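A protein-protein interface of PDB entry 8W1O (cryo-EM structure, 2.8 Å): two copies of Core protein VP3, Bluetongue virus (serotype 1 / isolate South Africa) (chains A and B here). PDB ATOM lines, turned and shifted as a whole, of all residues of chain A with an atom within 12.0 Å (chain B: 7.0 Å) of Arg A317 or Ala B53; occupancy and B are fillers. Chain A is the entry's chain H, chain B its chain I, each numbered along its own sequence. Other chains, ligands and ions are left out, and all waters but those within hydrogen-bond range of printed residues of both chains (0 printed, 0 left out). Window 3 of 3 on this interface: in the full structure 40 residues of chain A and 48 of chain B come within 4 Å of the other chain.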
ATOM      1  N   SER A 311      38.865  -1.050 -21.024  1.00  0.00           N
ATOM      2  CA  SER A 311      37.511  -1.580 -21.091  1.00  0.00           C
ATOM      3  C   SER A 311      37.433  -2.685 -22.135  1.00  0.00           C
ATOM      4  O   SER A 311      37.987  -2.554 -23.228  1.00  0.00           O
ATOM      5  CB  SER A 311      36.501  -0.476 -21.419  1.00  0.00           C
ATOM      6  OG  SER A 311      35.176  -0.975 -21.406  1.00  0.00           O
ATOM      7  N   ILE A 312      36.734  -3.767 -21.791  1.00  0.00           N
ATOM      8  CA  ILE A 312      36.557  -4.921 -22.665  1.00  0.00           C
ATOM      9  C   ILE A 312      35.069  -5.232 -22.766  1.00  0.00           C
ATOM     10  O   ILE A 312      34.375  -5.317 -21.749  1.00  0.00           O
ATOM     11  CB  ILE A 312      37.335  -6.148 -22.144  1.00  0.00           C
ATOM     12  CG1 ILE A 312      38.826  -6.011 -22.448  1.00  0.00           C
ATOM     13  CG2 ILE A 312      36.796  -7.434 -22.746  1.00  0.00           C
ATOM     14  CD1 ILE A 312      39.678  -7.039 -21.744  1.00  0.00           C
ATOM     15  N   THR A 313      34.585  -5.403 -23.994  1.00  0.00           N
ATOM     16  CA  THR A 313      33.196  -5.763 -24.249  1.00  0.00           C
ATOM     17  C   THR A 313      33.115  -7.246 -24.595  1.00  0.00           C
ATOM     18  O   THR A 313      33.788  -7.707 -25.523  1.00  0.00           O
ATOM     19  CB  THR A 313      32.614  -4.920 -25.385  1.00  0.00           C
ATOM     20  OG1 THR A 313      32.697  -3.531 -25.044  1.00  0.00           O
ATOM     21  CG2 THR A 313      31.165  -5.290 -25.636  1.00  0.00           C
ATOM     22  N   LEU A 314      32.294  -7.985 -23.851  1.00  0.00           N
ATOM     23  CA  LEU A 314      32.080  -9.408 -24.091  1.00  0.00           C
ATOM     24  C   LEU A 314      30.798  -9.679 -24.867  1.00  0.00           C
ATOM     25  O   LEU A 314      30.837 -10.311 -25.926  1.00  0.00           O
ATOM     26  CB  LEU A 314      32.057 -10.172 -22.763  1.00  0.00           C
ATOM     27  CG  LEU A 314      33.364 -10.212 -21.969  1.00  0.00           C
ATOM     28  CD1 LEU A 314      33.178 -10.976 -20.671  1.00  0.00           C
ATOM     29  CD2 LEU A 314      34.475 -10.828 -22.796  1.00  0.00           C
ATOM     30  N   THR A 315      29.658  -9.215 -24.358  1.00  0.00           N
ATOM     31  CA  THR A 315      28.395  -9.302 -25.081  1.00  0.00           C
ATOM     32  C   THR A 315      27.787  -7.911 -25.202  1.00  0.00           C
ATOM     33  O   THR A 315      28.437  -6.918 -24.868  1.00  0.00           O
ATOM     34  CB  THR A 315      27.416 -10.255 -24.385  1.00  0.00           C
ATOM     35  OG1 THR A 315      27.000  -9.693 -23.135  1.00  0.00           O
ATOM     36  CG2 THR A 315      28.056 -11.612 -24.138  1.00  0.00           C
ATOM     37  N   GLN A 316      26.542  -7.825 -25.675  1.00  0.00           N
ATOM     38  CA  GLN A 316      25.904  -6.520 -25.824  1.00  0.00           C
ATOM     39  C   GLN A 316      25.581  -5.884 -24.479  1.00  0.00           C
ATOM     40  O   GLN A 316      25.378  -4.667 -24.405  1.00  0.00           O
ATOM     41  CB  GLN A 316      24.633  -6.644 -26.664  1.00  0.00           C
ATOM     42  CG  GLN A 316      24.848  -6.399 -28.146  1.00  0.00           C
ATOM     43  CD  GLN A 316      23.566  -6.492 -28.947  1.00  0.00           C
ATOM     44  OE1 GLN A 316      22.469  -6.384 -28.399  1.00  0.00           O
ATOM     45  NE2 GLN A 316      23.699  -6.690 -30.253  1.00  0.00           N
ATOM     46  N   ARG A 317      25.532  -6.677 -23.407  1.00  0.00           N
ATOM     47  CA  ARG A 317      25.128  -6.173 -22.103  1.00  0.00           C
ATOM     48  C   ARG A 317      26.183  -6.335 -21.019  1.00  0.00           C
ATOM     49  O   ARG A 317      25.985  -5.824 -19.913  1.00  0.00           O
ATOM     50  CB  ARG A 317      23.833  -6.865 -21.651  1.00  0.00           C
ATOM     51  CG  ARG A 317      22.616  -6.454 -22.459  1.00  0.00           C
ATOM     52  CD  ARG A 317      21.329  -7.011 -21.883  1.00  0.00           C
ATOM     53  NE  ARG A 317      20.171  -6.282 -22.384  1.00  0.00           N
ATOM     54  CZ  ARG A 317      18.917  -6.703 -22.292  1.00  0.00           C
ATOM     55  NH1 ARG A 317      18.613  -7.846 -21.700  1.00  0.00           N
ATOM     56  NH2 ARG A 317      17.944  -5.958 -22.807  1.00  0.00           N
ATOM     57  N   ILE A 318      27.290  -7.017 -21.295  1.00  0.00           N
ATOM     58  CA  ILE A 318      28.317  -7.293 -20.298  1.00  0.00           C
ATOM     59  C   ILE A 318      29.607  -6.613 -20.733  1.00  0.00           C
ATOM     60  O   ILE A 318      30.070  -6.814 -21.861  1.00  0.00           O
ATOM     61  CB  ILE A 318      28.524  -8.805 -20.105  1.00  0.00           C
ATOM     62  CG1 ILE A 318      27.243  -9.445 -19.565  1.00  0.00           C
ATOM     63  CG2 ILE A 318      29.685  -9.070 -19.164  1.00  0.00           C
ATOM     64  CD1 ILE A 318      27.270 -10.954 -19.542  1.00  0.00           C
ATOM     65  N   THR A 319      30.183  -5.811 -19.839  1.00  0.00           N
ATOM     66  CA  THR A 319      31.358  -5.012 -20.149  1.00  0.00           C
ATOM     67  C   THR A 319      32.122  -4.731 -18.862  1.00  0.00           C
ATOM     68  O   THR A 319      31.530  -4.372 -17.841  1.00  0.00           O
ATOM     69  CB  THR A 319      30.964  -3.696 -20.839  1.00  0.00           C
ATOM     70  OG1 THR A 319      30.416  -3.976 -22.132  1.00  0.00           O
ATOM     71  CG2 THR A 319      32.164  -2.781 -21.002  1.00  0.00           C
ATOM     72  N   THR A 320      33.442  -4.901 -18.917  1.00  0.00           N
ATOM     73  CA  THR A 320      34.293  -4.616 -17.772  1.00  0.00           C
ATOM     74  C   THR A 320      34.407  -3.109 -17.544  1.00  0.00           C
ATOM     75  O   THR A 320      34.189  -2.297 -18.445  1.00  0.00           O
ATOM     76  CB  THR A 320      35.686  -5.213 -17.966  1.00  0.00           C
ATOM     77  OG1 THR A 320      36.331  -4.579 -19.076  1.00  0.00           O
ATOM     78  CG2 THR A 320      35.595  -6.702 -18.229  1.00  0.00           C
ATOM     79  N   THR A 321      34.759  -2.743 -16.313  1.00  0.00           N
ATOM     80  CA  THR A 321      34.874  -1.348 -15.908  1.00  0.00           C
ATOM     81  C   THR A 321      36.228  -1.098 -15.259  1.00  0.00           C
ATOM     82  O   THR A 321      36.827  -1.999 -14.665  1.00  0.00           O
ATOM     83  CB  THR A 321      33.759  -0.945 -14.929  1.00  0.00           C
ATOM     84  OG1 THR A 321      33.851  -1.739 -13.740  1.00  0.00           O
ATOM     85  CG2 THR A 321      32.387  -1.131 -15.561  1.00  0.00           C
ATOM     86  N   GLN B  47       7.272   1.705 -20.343  1.00  0.00           N
ATOM     87  CA  GLN B  47       6.871   0.320 -20.580  1.00  0.00           C
ATOM     88  C   GLN B  47       7.786  -0.349 -21.598  1.00  0.00           C
ATOM     89  O   GLN B  47       8.212  -1.498 -21.414  1.00  0.00           O
ATOM     90  CB  GLN B  47       5.422   0.267 -21.061  1.00  0.00           C
ATOM     91  CG  GLN B  47       4.378   0.364 -19.968  1.00  0.00           C
ATOM     92  CD  GLN B  47       2.971   0.352 -20.525  1.00  0.00           C
ATOM     93  OE1 GLN B  47       2.657   1.081 -21.464  1.00  0.00           O
ATOM     94  NE2 GLN B  47       2.116  -0.485 -19.954  1.00  0.00           N
ATOM     95  N   ALA B  48       8.094   0.361 -22.688  1.00  0.00           N
ATOM     96  CA  ALA B  48       8.982  -0.190 -23.709  1.00  0.00           C
ATOM     97  C   ALA B  48      10.378  -0.436 -23.156  1.00  0.00           C
ATOM     98  O   ALA B  48      11.009  -1.457 -23.464  1.00  0.00           O
ATOM     99  CB  ALA B  48       9.039   0.748 -24.914  1.00  0.00           C
ATOM    100  N   ASP B  49      10.881   0.495 -22.341  1.00  0.00           N
ATOM    101  CA  ASP B  49      12.195   0.311 -21.729  1.00  0.00           C
ATOM    102  C   ASP B  49      12.211  -0.903 -20.808  1.00  0.00           C
ATOM    103  O   ASP B  49      13.172  -1.682 -20.816  1.00  0.00           O
ATOM    104  CB  ASP B  49      12.603   1.570 -20.967  1.00  0.00           C
ATOM    105  CG  ASP B  49      12.670   2.794 -21.857  1.00  0.00           C
ATOM    106  OD1 ASP B  49      12.598   2.635 -23.093  1.00  0.00           O
ATOM    107  OD2 ASP B  49      12.790   3.915 -21.321  1.00  0.00           O
ATOM    108  N   TYR B  50      11.156  -1.088 -20.011  1.00  0.00           N
ATOM    109  CA  TYR B  50      11.105  -2.260 -19.141  1.00  0.00           C
ATOM    110  C   TYR B  50      11.064  -3.550 -19.952  1.00  0.00           C
ATOM    111  O   TYR B  50      11.757  -4.523 -19.620  1.00  0.00           O
ATOM    112  CB  TYR B  50       9.900  -2.185 -18.208  1.00  0.00           C
ATOM    113  CG  TYR B  50       9.824  -3.355 -17.256  1.00  0.00           C
ATOM    114  CD1 TYR B  50      10.664  -3.433 -16.154  1.00  0.00           C
ATOM    115  CD2 TYR B  50       8.930  -4.393 -17.472  1.00  0.00           C
ATOM    116  CE1 TYR B  50      10.604  -4.504 -15.285  1.00  0.00           C
ATOM    117  CE2 TYR B  50       8.862  -5.465 -16.609  1.00  0.00           C
ATOM    118  CZ  TYR B  50       9.700  -5.518 -15.518  1.00  0.00           C
ATOM    119  OH  TYR B  50       9.633  -6.588 -14.658  1.00  0.00           O
ATOM    120  N   MET B  51      10.260  -3.578 -21.020  1.00  0.00           N
ATOM    121  CA  MET B  51      10.181  -4.786 -21.837  1.00  0.00           C
ATOM    122  C   MET B  51      11.516  -5.109 -22.492  1.00  0.00           C
ATOM    123  O   MET B  51      11.930  -6.272 -22.514  1.00  0.00           O
ATOM    124  CB  MET B  51       9.084  -4.669 -22.896  1.00  0.00           C
ATOM    125  CG  MET B  51       7.673  -4.617 -22.341  1.00  0.00           C
ATOM    126  SD  MET B  51       6.420  -4.551 -23.638  1.00  0.00           S
ATOM    127  CE  MET B  51       6.585  -2.866 -24.210  1.00  0.00           C
ATOM    128  N   THR B  52      12.215  -4.101 -23.023  1.00  0.00           N
ATOM    129  CA  THR B  52      13.494  -4.395 -23.664  1.00  0.00           C
ATOM    130  C   THR B  52      14.563  -4.735 -22.631  1.00  0.00           C
ATOM    131  O   THR B  52      15.545  -5.414 -22.951  1.00  0.00           O
ATOM    132  CB  THR B  52      13.946  -3.232 -24.553  1.00  0.00           C
ATOM    133  OG1 THR B  52      15.108  -3.624 -25.293  1.00  0.00           O
ATOM    134  CG2 THR B  52      14.295  -2.011 -23.731  1.00  0.00           C
ATOM    135  N   ALA B  53      14.391  -4.280 -21.385  1.00  0.00           N
ATOM    136  CA  ALA B  53      15.326  -4.663 -20.333  1.00  0.00           C
ATOM    137  C   ALA B  53      15.144  -6.123 -19.934  1.00  0.00           C
ATOM    138  O   ALA B  53      16.126  -6.847 -19.738  1.00  0.00           O
ATOM    139  CB  ALA B  53      15.156  -3.750 -19.121  1.00  0.00           C
ATOM    140  N   THR B  54      13.893  -6.576 -19.808  1.00  0.00           N
ATOM    141  CA  THR B  54      13.659  -7.937 -19.331  1.00  0.00           C
ATOM    142  C   THR B  54      13.737  -8.966 -20.455  1.00  0.00           C
ATOM    143  O   THR B  54      13.721 -10.173 -20.188  1.00  0.00           O
ATOM    144  CB  THR B  54      12.302  -8.026 -18.636  1.00  0.00           C
ATOM    145  OG1 THR B  54      12.160  -9.315 -18.027  1.00  0.00           O
ATOM    146  CG2 THR B  54      11.182  -7.822 -19.639  1.00  0.00           C
ATOM    147  N   ARG B  55      13.820  -8.520 -21.704  1.00  0.00           N
ATOM    148  CA  ARG B  55      13.728  -9.422 -22.842  1.00  0.00           C
ATOM    149  C   ARG B  55      15.067 -10.114 -23.104  1.00  0.00           C
ATOM    150  O   ARG B  55      16.138  -9.571 -22.821  1.00  0.00           O
ATOM    151  CB  ARG B  55      13.256  -8.637 -24.067  1.00  0.00           C
ATOM    152  CG  ARG B  55      12.958  -9.436 -25.310  1.00  0.00           C
ATOM    153  CD  ARG B  55      14.087  -9.284 -26.290  1.00  0.00           C
ATOM    154  NE  ARG B  55      14.402  -7.885 -26.549  1.00  0.00           N
ATOM    155  CZ  ARG B  55      15.612  -7.435 -26.850  1.00  0.00           C
ATOM    156  NH1 ARG B  55      16.651  -8.252 -26.929  1.00  0.00           N
ATOM    157  NH2 ARG B  55      15.785  -6.137 -27.076  1.00  0.00           N
ATOM    158  N   GLU B  56      14.996 -11.331 -23.647  1.00  0.00           N
ATOM    159  CA  GLU B  56      16.167 -12.173 -23.877  1.00  0.00           C
ATOM    160  C   GLU B  56      16.275 -12.526 -25.356  1.00  0.00           C
ATOM    161  O   GLU B  56      15.452 -13.285 -25.877  1.00  0.00           O
ATOM    162  CB  GLU B  56      16.096 -13.452 -23.040  1.00  0.00           C
ATOM    163  CG  GLU B  56      16.110 -13.236 -21.534  1.00  0.00           C
ATOM    164  CD  GLU B  56      17.469 -12.820 -21.015  1.00  0.00           C
ATOM    165  OE1 GLU B  56      18.482 -13.383 -21.479  1.00  0.00           O
ATOM    166  OE2 GLU B  56      17.523 -11.933 -20.138  1.00  0.00           O
ATOM    167  N   VAL B  57      17.297 -11.977 -26.021  1.00  0.00           N
ATOM    168  CA  VAL B  57      17.686 -12.340 -27.380  1.00  0.00           C
ATOM    169  C   VAL B  57      19.210 -12.415 -27.381  1.00  0.00           C
ATOM    170  O   VAL B  57      19.871 -11.878 -26.490  1.00  0.00           O
ATOM    171  CB  VAL B  57      17.133 -11.325 -28.430  1.00  0.00           C
ATOM    172  CG1 VAL B  57      17.704 -11.523 -29.830  1.00  0.00           C
ATOM    173  CG2 VAL B  57      15.631 -11.447 -28.534  1.00  0.00           C
ATOM    174  N   PHE B  59      22.870 -11.723 -27.660  1.00  0.00           N
ATOM    175  CA  PHE B  59      23.457 -10.434 -27.321  1.00  0.00           C
ATOM    176  C   PHE B  59      24.853 -10.257 -27.910  1.00  0.00           C
ATOM    177  O   PHE B  59      25.725  -9.656 -27.279  1.00  0.00           O
ATOM    178  CB  PHE B  59      23.500 -10.267 -25.803  1.00  0.00           C
ATOM    179  CG  PHE B  59      22.149 -10.102 -25.176  1.00  0.00           C
ATOM    180  CD1 PHE B  59      21.249  -9.174 -25.673  1.00  0.00           C
ATOM    181  CD2 PHE B  59      21.782 -10.868 -24.081  1.00  0.00           C
ATOM    182  CE1 PHE B  59      20.005  -9.019 -25.096  1.00  0.00           C
ATOM    183  CE2 PHE B  59      20.537 -10.719 -23.500  1.00  0.00           C
ATOM    184  CZ  PHE B  59      19.649  -9.794 -24.009  1.00  0.00           C
ATOM    185  N   VAL B  61      27.844  -8.750 -30.144  1.00  0.00           N
ATOM    186  CA  VAL B  61      28.194  -7.399 -30.595  1.00  0.00           C
ATOM    187  C   VAL B  61      28.078  -7.334 -32.112  1.00  0.00           C
ATOM    188  O   VAL B  61      28.537  -8.263 -32.801  1.00  0.00           O
ATOM    189  CB  VAL B  61      29.608  -7.039 -30.130  1.00  0.00           C
ATOM    190  CG1 VAL B  61      29.892  -5.563 -30.336  1.00  0.00           C
ATOM    191  CG2 VAL B  61      29.794  -7.424 -28.671  1.00  0.00           C
ATOM    192  N   ALA B 334      16.647  -4.381 -13.119  1.00  0.00           N
ATOM    193  CA  ALA B 334      17.376  -4.671 -14.351  1.00  0.00           C
ATOM    194  C   ALA B 334      18.857  -4.915 -14.084  1.00  0.00           C
ATOM    195  O   ALA B 334      19.457  -5.836 -14.656  1.00  0.00           O
ATOM    196  CB  ALA B 334      17.190  -3.528 -15.347  1.00  0.00           C
ATOM    197  N   LEU B 337      19.434  -8.320 -12.595  1.00  0.00           N
ATOM    198  CA  LEU B 337      19.309  -9.328 -13.645  1.00  0.00           C
ATOM    199  C   LEU B 337      20.574  -9.404 -14.495  1.00  0.00           C
ATOM    200  O   LEU B 337      21.035 -10.499 -14.849  1.00  0.00           O
ATOM    201  CB  LEU B 337      18.094  -9.017 -14.516  1.00  0.00           C
ATOM    202  CG  LEU B 337      17.314 -10.204 -15.081  1.00  0.00           C
ATOM    203  CD1 LEU B 337      16.850 -11.127 -13.969  1.00  0.00           C
ATOM    204  CD2 LEU B 337      16.137  -9.714 -15.901  1.00  0.00           C
ATOM    205  N   ASN B 338      21.151  -8.247 -14.831  1.00  0.00           N
ATOM    206  CA  ASN B 338      22.412  -8.239 -15.568  1.00  0.00           C
ATOM    207  C   ASN B 338      23.528  -8.887 -14.757  1.00  0.00           C
ATOM    208  O   ASN B 338      24.390  -9.581 -15.309  1.00  0.00           O
ATOM    209  CB  ASN B 338      22.783  -6.807 -15.950  1.00  0.00           C
ATOM    210  CG  ASN B 338      23.466  -6.723 -17.297  1.00  0.00           C
ATOM    211  OD1 ASN B 338      23.031  -7.341 -18.267  1.00  0.00           O
ATOM    212  ND2 ASN B 338      24.544  -5.955 -17.364  1.00  0.00           N
ATOM    213  N   ARG B 341      23.190 -12.542 -15.095  1.00  0.00           N
ATOM    214  CA  ARG B 341      23.758 -12.948 -16.379  1.00  0.00           C
ATOM    215  C   ARG B 341      25.278 -13.037 -16.308  1.00  0.00           C
ATOM    216  O   ARG B 341      25.883 -13.971 -16.853  1.00  0.00           O
ATOM    217  CB  ARG B 341      23.340 -11.972 -17.477  1.00  0.00           C
ATOM    218  CG  ARG B 341      21.853 -11.920 -17.748  1.00  0.00           C
ATOM    219  CD  ARG B 341      21.555 -10.988 -18.907  1.00  0.00           C
ATOM    220  NE  ARG B 341      20.125 -10.819 -19.126  1.00  0.00           N
ATOM    221  CZ  ARG B 341      19.479  -9.670 -18.986  1.00  0.00           C
ATOM    222  NH1 ARG B 341      20.106  -8.562 -18.632  1.00  0.00           N
ATOM    223  NH2 ARG B 341      18.168  -9.633 -19.211  1.00  0.00           N
ATOM    224  N   LYS B 342      25.913 -12.072 -15.636  1.00  0.00           N
ATOM    225  CA  LYS B 342      27.363 -12.114 -15.449  1.00  0.00           C
ATOM    226  C   LYS B 342      27.789 -13.342 -14.653  1.00  0.00           C
ATOM    227  O   LYS B 342      28.809 -13.970 -14.964  1.00  0.00           O
ATOM    228  CB  LYS B 342      27.847 -10.850 -14.744  1.00  0.00           C
ATOM    229  CG  LYS B 342      27.656  -9.570 -15.521  1.00  0.00           C
ATOM    230  CD  LYS B 342      28.241  -8.402 -14.761  1.00  0.00           C
ATOM    231  CE  LYS B 342      28.064  -7.102 -15.516  1.00  0.00           C
ATOM    232  NZ  LYS B 342      28.519  -5.946 -14.701  1.00  0.00           N
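The side-chain hydroxyl of Thr A315 lies close to the backbone NH of Arg A317 (3.4 Å). The side-chain hydroxyl (OG1) of Thr A315 is in hydrogen-bond range of the backbone NH (N) of Ile A318. OG1 of Thr B52 is in hydrogen-bond range of NH2 of Arg B55. O of Ala B53 is in hydrogen-bond range of NH2 of Arg B341 (3.5 Å). The guanidinium group (NH2) of Arg B341 is in salt-bridge range of the side-chain carboxylate (OE2) of Glu B56 (2.6 Å). OD1 of Asn B338 lies within hydrogen-bond range of NH1 of Arg B341, 3.2 Å away.
No position is printed for both chains. Of the 9 pairs that touch across the chains among the printed residues, none has its exchanged pair printed and touching as well.
Of the 11 printed residues of chain A, 4 touch a printed residue of chain B. Among the printed residues, 9 pairs touch across the chains.
The backbone NH (N) of Gln A316 sits at hydrogen-bond distance from the backbone carbonyl oxygen (O) of Phe B59, at 2.6 Å. The guanidinium group of Arg A317 sits at hydrogen-bond distance from the backbone carbonyl oxygen of Thr B52, at 2.5 Å. NH1 of Arg A317 is in hydrogen-bond range of O of Ala B53 (3.3 Å). The guanidinium group (NH1) of Arg A317 lies within hydrogen-bond range of the backbone carbonyl oxygen (O) of Arg B55, at 3.2 Å. ND2 of Asn B338 is in hydrogen-bond range of O of Arg A317, at 2.9 Å. The guanidinium group (NH1) of Arg A317 sits close to the guanidinium group (NH2) of Arg B341 (3.1 Å).
Among the printed residues, pairs that only touch across the chains: Arg A317 with Phe B59, Thr A315 with Phe B59 and Thr A313 with Val B61.
Arg A317 touches six residues of chain B. Ala B53 touches just one residue of chain A: Arg A317 (3.3 Å). No residue of chain A comes within 4 Å of Tyr B50. Thr B52 touches just one residue of chain A: Arg A317 (2.5 Å). No residue of chain A comes within 4 Å of Glu B56. Phe B59 touches three residues of chain A. Asn B338 touches just one residue of chain A: Arg A317 (2.9 Å). Of the printed residues of chain B, Thr A313 touches Val B61. Printed residues of chain B within 4 Å of Thr A315: Phe B59. Of the printed residues of chain A, Val B61 touches Thr A313. Of the printed residues of chain B, Gln A316 touches Phe B59 (2.6 Å). The nearest residue of chain B that does not touch Arg A317 is Glu B56 (4.5 Å). The nearest printed residue of chain B that does not touch Gln A316 is Val B61 (4.3 Å).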
